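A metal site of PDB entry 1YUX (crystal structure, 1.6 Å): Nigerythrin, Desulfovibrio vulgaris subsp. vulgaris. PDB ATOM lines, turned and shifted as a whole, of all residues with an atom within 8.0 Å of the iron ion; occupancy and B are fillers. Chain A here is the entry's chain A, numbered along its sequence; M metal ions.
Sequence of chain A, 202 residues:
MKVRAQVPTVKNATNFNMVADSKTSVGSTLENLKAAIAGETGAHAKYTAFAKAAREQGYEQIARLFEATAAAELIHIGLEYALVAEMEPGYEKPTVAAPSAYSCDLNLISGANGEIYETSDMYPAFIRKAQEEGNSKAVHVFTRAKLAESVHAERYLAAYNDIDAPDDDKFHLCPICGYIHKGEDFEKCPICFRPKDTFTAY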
ATOM      1  N   ILE A  75      -6.254   7.844 -21.108  1.00  0.00           N
ATOM      2  CA  ILE A  75      -7.570   7.410 -21.559  1.00  0.00           C
ATOM      3  C   ILE A  75      -7.364   6.753 -22.929  1.00  0.00           C
ATOM      4  O   ILE A  75      -7.919   5.691 -23.206  1.00  0.00           O
ATOM      5  CB  ILE A  75      -8.544   8.603 -21.690  1.00  0.00           C
ATOM      6  CG1 ILE A  75      -8.957   9.082 -20.294  1.00  0.00           C
ATOM      7  CG2 ILE A  75      -9.774   8.197 -22.507  1.00  0.00           C
ATOM      8  CD1 ILE A  75      -9.844  10.311 -20.306  1.00  0.00           C
ATOM      9  N   ARG A 144     -11.299   8.608 -32.273  1.00  0.00           N
ATOM     10  CA  ARG A 144     -11.522   9.310 -31.022  1.00  0.00           C
ATOM     11  C   ARG A 144     -10.235   9.958 -30.530  1.00  0.00           C
ATOM     12  O   ARG A 144     -10.231  11.126 -30.145  1.00  0.00           O
ATOM     13  CB  ARG A 144     -12.064   8.325 -29.972  1.00  0.00           C
ATOM     14  CG  ARG A 144     -12.476   8.968 -28.665  1.00  0.00           C
ATOM     15  CD  ARG A 144     -13.676   8.250 -28.061  1.00  0.00           C
ATOM     16  NE  ARG A 144     -14.881   8.445 -28.863  1.00  0.00           N
ATOM     17  CZ  ARG A 144     -16.097   8.053 -28.510  1.00  0.00           C
ATOM     18  NH1 ARG A 144     -16.282   7.415 -27.354  1.00  0.00           N
ATOM     19  NH2 ARG A 144     -17.135   8.297 -29.296  1.00  0.00           N
ATOM     20  N   ALA A 148      -9.029  14.213 -30.286  1.00  0.00           N
ATOM     21  CA  ALA A 148      -8.595  14.838 -29.056  1.00  0.00           C
ATOM     22  C   ALA A 148      -7.226  15.510 -29.192  1.00  0.00           C
ATOM     23  O   ALA A 148      -6.980  16.561 -28.601  1.00  0.00           O
ATOM     24  CB  ALA A 148      -8.544  13.810 -27.932  1.00  0.00           C
ATOM     25  N   LEU A 173     -11.635  17.347 -18.251  1.00  0.00           N
ATOM     26  CA  LEU A 173     -11.342  16.205 -19.111  1.00  0.00           C
ATOM     27  C   LEU A 173     -12.537  15.276 -19.217  1.00  0.00           C
ATOM     28  O   LEU A 173     -13.165  14.933 -18.210  1.00  0.00           O
ATOM     29  CB  LEU A 173     -10.148  15.429 -18.543  1.00  0.00           C
ATOM     30  CG  LEU A 173      -9.736  14.150 -19.277  1.00  0.00           C
ATOM     31  CD1 LEU A 173      -9.309  14.502 -20.703  1.00  0.00           C
ATOM     32  CD2 LEU A 173      -8.606  13.479 -18.520  1.00  0.00           C
ATOM     33  N   CYS A 174     -12.848  14.876 -20.443  1.00  0.00           N
ATOM     34  CA  CYS A 174     -13.958  13.962 -20.702  1.00  0.00           C
ATOM     35  C   CYS A 174     -13.635  12.603 -20.072  1.00  0.00           C
ATOM     36  O   CYS A 174     -12.484  12.216 -20.002  1.00  0.00           O
ATOM     37  CB  CYS A 174     -14.157  13.815 -22.214  1.00  0.00           C
ATOM     38  SG  CYS A 174     -15.446  12.632 -22.680  1.00  0.00           S
ATOM     39  N   PRO A 175     -14.663  11.880 -19.614  1.00  0.00           N
ATOM     40  CA  PRO A 175     -14.444  10.565 -19.000  1.00  0.00           C
ATOM     41  C   PRO A 175     -14.035   9.439 -19.936  1.00  0.00           C
ATOM     42  O   PRO A 175     -13.332   8.511 -19.525  1.00  0.00           O
ATOM     43  CB  PRO A 175     -15.779  10.285 -18.314  1.00  0.00           C
ATOM     44  CG  PRO A 175     -16.768  10.959 -19.215  1.00  0.00           C
ATOM     45  CD  PRO A 175     -16.084  12.281 -19.502  1.00  0.00           C
ATOM     46  N   ILE A 176     -14.444   9.517 -21.202  1.00  0.00           N
ATOM     47  CA  ILE A 176     -14.124   8.457 -22.142  1.00  0.00           C
ATOM     48  C   ILE A 176     -13.285   8.821 -23.369  1.00  0.00           C
ATOM     49  O   ILE A 176     -12.958   7.948 -24.177  1.00  0.00           O
ATOM     50  CB  ILE A 176     -15.410   7.739 -22.616  1.00  0.00           C
ATOM     51  CG1 ILE A 176     -16.299   8.722 -23.373  1.00  0.00           C
ATOM     52  CG2 ILE A 176     -16.154   7.178 -21.399  1.00  0.00           C
ATOM     53  CD1 ILE A 176     -17.547   8.083 -23.980  1.00  0.00           C
ATOM     54  N   CYS A 177     -12.951  10.094 -23.518  1.00  0.00           N
ATOM     55  CA  CYS A 177     -12.102  10.511 -24.636  1.00  0.00           C
ATOM     56  C   CYS A 177     -11.166  11.587 -24.121  1.00  0.00           C
ATOM     57  O   CYS A 177     -11.314  12.064 -22.989  1.00  0.00           O
ATOM     58  CB  CYS A 177     -12.942  11.001 -25.833  1.00  0.00           C
ATOM     59  SG  CYS A 177     -13.450  12.726 -25.849  1.00  0.00           S
ATOM     60  N   GLY A 178     -10.195  11.981 -24.938  1.00  0.00           N
ATOM     61  CA  GLY A 178      -9.223  12.971 -24.500  1.00  0.00           C
ATOM     62  C   GLY A 178      -9.615  14.429 -24.575  1.00  0.00           C
ATOM     63  O   GLY A 178      -8.777  15.306 -24.373  1.00  0.00           O
ATOM     64  N   TYR A 179     -10.883  14.711 -24.847  1.00  0.00           N
ATOM     65  CA  TYR A 179     -11.304  16.100 -24.947  1.00  0.00           C
ATOM     66  C   TYR A 179     -11.083  16.874 -23.657  1.00  0.00           C
ATOM     67  O   TYR A 179     -11.392  16.387 -22.569  1.00  0.00           O
ATOM     68  CB  TYR A 179     -12.782  16.185 -25.324  1.00  0.00           C
ATOM     69  CG  TYR A 179     -13.282  17.607 -25.368  1.00  0.00           C
ATOM     70  CD1 TYR A 179     -12.873  18.482 -26.366  1.00  0.00           C
ATOM     71  CD2 TYR A 179     -14.159  18.078 -24.388  1.00  0.00           C
ATOM     72  CE1 TYR A 179     -13.315  19.806 -26.392  1.00  0.00           C
ATOM     73  CE2 TYR A 179     -14.599  19.396 -24.401  1.00  0.00           C
ATOM     74  CZ  TYR A 179     -14.190  20.246 -25.405  1.00  0.00           C
ATOM     75  OH  TYR A 179     -14.654  21.545 -25.424  1.00  0.00           O
ATOM     76  N   ILE A 180     -10.550  18.078 -23.787  1.00  0.00           N
ATOM     77  CA  ILE A 180     -10.290  18.948 -22.647  1.00  0.00           C
ATOM     78  C   ILE A 180     -10.866  20.323 -22.940  1.00  0.00           C
ATOM     79  O   ILE A 180     -10.653  20.874 -24.018  1.00  0.00           O
ATOM     80  CB  ILE A 180      -8.783  19.119 -22.387  1.00  0.00           C
ATOM     81  CG1 ILE A 180      -8.195  17.799 -21.894  1.00  0.00           C
ATOM     82  CG2 ILE A 180      -8.532  20.233 -21.364  1.00  0.00           C
ATOM     83  CD1 ILE A 180      -6.680  17.791 -21.824  1.00  0.00           C
ATOM     84  N   LYS A 188     -21.330  19.831 -23.320  1.00  0.00           N
ATOM     85  CA  LYS A 188     -20.954  18.432 -23.495  1.00  0.00           C
ATOM     86  C   LYS A 188     -19.728  18.296 -24.374  1.00  0.00           C
ATOM     87  O   LYS A 188     -19.298  19.256 -25.012  1.00  0.00           O
ATOM     88  CB  LYS A 188     -22.114  17.655 -24.110  1.00  0.00           C
ATOM     89  CG  LYS A 188     -22.514  18.151 -25.491  1.00  0.00           C
ATOM     90  CD  LYS A 188     -23.588  17.273 -26.102  1.00  0.00           C
ATOM     91  CE  LYS A 188     -23.968  17.771 -27.494  1.00  0.00           C
ATOM     92  NZ  LYS A 188     -24.988  16.895 -28.146  1.00  0.00           N
ATOM     93  N   CYS A 189     -19.174  17.087 -24.402  1.00  0.00           N
ATOM     94  CA  CYS A 189     -17.992  16.797 -25.195  1.00  0.00           C
ATOM     95  C   CYS A 189     -18.343  16.813 -26.683  1.00  0.00           C
ATOM     96  O   CYS A 189     -19.276  16.140 -27.109  1.00  0.00           O
ATOM     97  CB  CYS A 189     -17.435  15.430 -24.812  1.00  0.00           C
ATOM     98  SG  CYS A 189     -15.940  14.968 -25.711  1.00  0.00           S
ATOM     99  N   PRO A 190     -17.601  17.599 -27.484  1.00  0.00           N
ATOM    100  CA  PRO A 190     -17.863  17.689 -28.922  1.00  0.00           C
ATOM    101  C   PRO A 190     -17.378  16.468 -29.710  1.00  0.00           C
ATOM    102  O   PRO A 190     -17.691  16.318 -30.896  1.00  0.00           O
ATOM    103  CB  PRO A 190     -17.131  18.962 -29.325  1.00  0.00           C
ATOM    104  CG  PRO A 190     -15.958  18.957 -28.406  1.00  0.00           C
ATOM    105  CD  PRO A 190     -16.564  18.557 -27.083  1.00  0.00           C
ATOM    106  N   ILE A 191     -16.615  15.604 -29.046  1.00  0.00           N
ATOM    107  CA  ILE A 191     -16.088  14.413 -29.678  1.00  0.00           C
ATOM    108  C   ILE A 191     -16.969  13.185 -29.430  1.00  0.00           C
ATOM    109  O   ILE A 191     -17.227  12.414 -30.354  1.00  0.00           O
ATOM    110  CB  ILE A 191     -14.648  14.100 -29.175  1.00  0.00           C
ATOM    111  CG1 ILE A 191     -13.697  15.210 -29.637  1.00  0.00           C
ATOM    112  CG2 ILE A 191     -14.188  12.745 -29.706  1.00  0.00           C
ATOM    113  CD1 ILE A 191     -12.282  15.065 -29.120  1.00  0.00           C
ATOM    114  N   CYS A 192     -17.443  13.013 -28.200  1.00  0.00           N
ATOM    115  CA  CYS A 192     -18.279  11.854 -27.889  1.00  0.00           C
ATOM    116  C   CYS A 192     -19.635  12.206 -27.277  1.00  0.00           C
ATOM    117  O   CYS A 192     -20.445  11.319 -26.993  1.00  0.00           O
ATOM    118  CB  CYS A 192     -17.539  10.912 -26.938  1.00  0.00           C
ATOM    119  SG  CYS A 192     -17.319  11.588 -25.286  1.00  0.00           S
ATOM    120  N   PHE A 193     -19.884  13.494 -27.069  1.00  0.00           N
ATOM    121  CA  PHE A 193     -21.150  13.983 -26.528  1.00  0.00           C
ATOM    122  C   PHE A 193     -21.413  13.758 -25.036  1.00  0.00           C
ATOM    123  O   PHE A 193     -22.506  14.056 -24.546  1.00  0.00           O
ATOM    124  CB  PHE A 193     -22.317  13.435 -27.351  1.00  0.00           C
ATOM    125  CG  PHE A 193     -22.511  14.133 -28.672  1.00  0.00           C
ATOM    126  CD1 PHE A 193     -21.469  14.853 -29.265  1.00  0.00           C
ATOM    127  CD2 PHE A 193     -23.727  14.057 -29.351  1.00  0.00           C
ATOM    128  CE1 PHE A 193     -21.645  15.482 -30.496  1.00  0.00           C
ATOM    129  CE2 PHE A 193     -23.914  14.681 -30.575  1.00  0.00           C
ATOM    130  CZ  PHE A 193     -22.867  15.404 -31.159  1.00  0.00           C
ATOM    131  N   ARG A 194     -20.429  13.237 -24.311  1.00  0.00           N
ATOM    132  CA  ARG A 194     -20.585  13.016 -22.875  1.00  0.00           C
ATOM    133  C   ARG A 194     -20.926  14.328 -22.175  1.00  0.00           C
ATOM    134  O   ARG A 194     -20.317  15.363 -22.452  1.00  0.00           O
ATOM    135  CB  ARG A 194     -19.315  12.434 -22.272  1.00  0.00           C
ATOM    136  CG  ARG A 194     -19.276  10.923 -22.207  1.00  0.00           C
ATOM    137  CD  ARG A 194     -20.309  10.408 -21.211  1.00  0.00           C
ATOM    138  NE  ARG A 194     -20.159   8.977 -20.959  1.00  0.00           N
ATOM    139  CZ  ARG A 194     -20.462   8.020 -21.823  1.00  0.00           C
ATOM    140  NH1 ARG A 194     -20.954   8.325 -23.024  1.00  0.00           N
ATOM    141  NH2 ARG A 194     -20.285   6.744 -21.498  1.00  0.00           N
ATOM    142  N   PRO A 195     -21.919  14.310 -21.272  1.00  0.00           N
ATOM    143  CA  PRO A 195     -22.332  15.510 -20.540  1.00  0.00           C
ATOM    144  C   PRO A 195     -21.216  16.089 -19.676  1.00  0.00           C
ATOM    145  O   PRO A 195     -20.355  15.364 -19.180  1.00  0.00           O
ATOM    146  CB  PRO A 195     -23.503  15.021 -19.710  1.00  0.00           C
ATOM    147  CG  PRO A 195     -24.087  13.936 -20.556  1.00  0.00           C
ATOM    148  CD  PRO A 195     -22.846  13.201 -21.008  1.00  0.00           C
ATOM    149  N   THR A 198     -19.972  14.692 -16.240  1.00  0.00           N
ATOM    150  CA  THR A 198     -19.236  13.430 -16.163  1.00  0.00           C
ATOM    151  C   THR A 198     -17.727  13.651 -16.300  1.00  0.00           C
ATOM    152  O   THR A 198     -16.944  12.711 -16.194  1.00  0.00           O
ATOM    153  CB  THR A 198     -19.690  12.444 -17.253  1.00  0.00           C
ATOM    154  OG1 THR A 198     -19.321  12.943 -18.549  1.00  0.00           O
ATOM    155  CG2 THR A 198     -21.198  12.254 -17.206  1.00  0.00           C
ATOM    156  N   PHE A 199     -17.338  14.903 -16.519  1.00  0.00           N
ATOM    157  CA  PHE A 199     -15.939  15.275 -16.661  1.00  0.00           C
ATOM    158  C   PHE A 199     -15.214  15.327 -15.327  1.00  0.00           C
ATOM    159  O   PHE A 199     -15.825  15.283 -14.257  1.00  0.00           O
ATOM    160  CB  PHE A 199     -15.825  16.655 -17.326  1.00  0.00           C
ATOM    161  CG  PHE A 199     -16.021  16.659 -18.822  1.00  0.00           C
ATOM    162  CD1 PHE A 199     -17.147  16.079 -19.393  1.00  0.00           C
ATOM    163  CD2 PHE A 199     -15.095  17.282 -19.653  1.00  0.00           C
ATOM    164  CE1 PHE A 199     -17.345  16.131 -20.773  1.00  0.00           C
ATOM    165  CE2 PHE A 199     -15.280  17.332 -21.028  1.00  0.00           C
ATOM    166  CZ  PHE A 199     -16.414  16.756 -21.595  1.00  0.00           C
HETATM  167 FE    FE M   1     -15.510  12.862 -24.929  1.00  0.00          FE
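The side-chain sulfur of Cys 192 lies close to the backbone NH of Arg 194, at 3.7 Å.
The side-chain sulfur (SG) of Cys 177 sits close to the backbone NH (N) of Tyr 179 (3.4 Å).
The backbone carbonyl oxygen (O) of Tyr 179 sits at hydrogen-bond distance from the backbone NH (N) of Cys 174, 3.0 Å away.
The side-chain sulfur (SG) of Cys 174 lies close to the backbone NH (N) of Ile 176 (3.6 Å).
N of Ile 191 sits close to SG of Cys 189 (3.5 Å).
The backbone carbonyl oxygen (O) of Arg 194 lies within hydrogen-bond range of the backbone NH (N) of Cys 189, 2.8 Å away.
Along chain A the residues within 4 Å of the iron ion span positions 174 to 192.
The iron ion is bound by the side-chain sulfur (SG) of Cys 192 (2.2 Å), the side-chain sulfur (SG) of Cys 177 (2.3 Å), the side-chain sulfur (SG) of Cys 174 (2.3 Å) and the side-chain sulfur (SG) of Cys 189 (2.3 Å).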
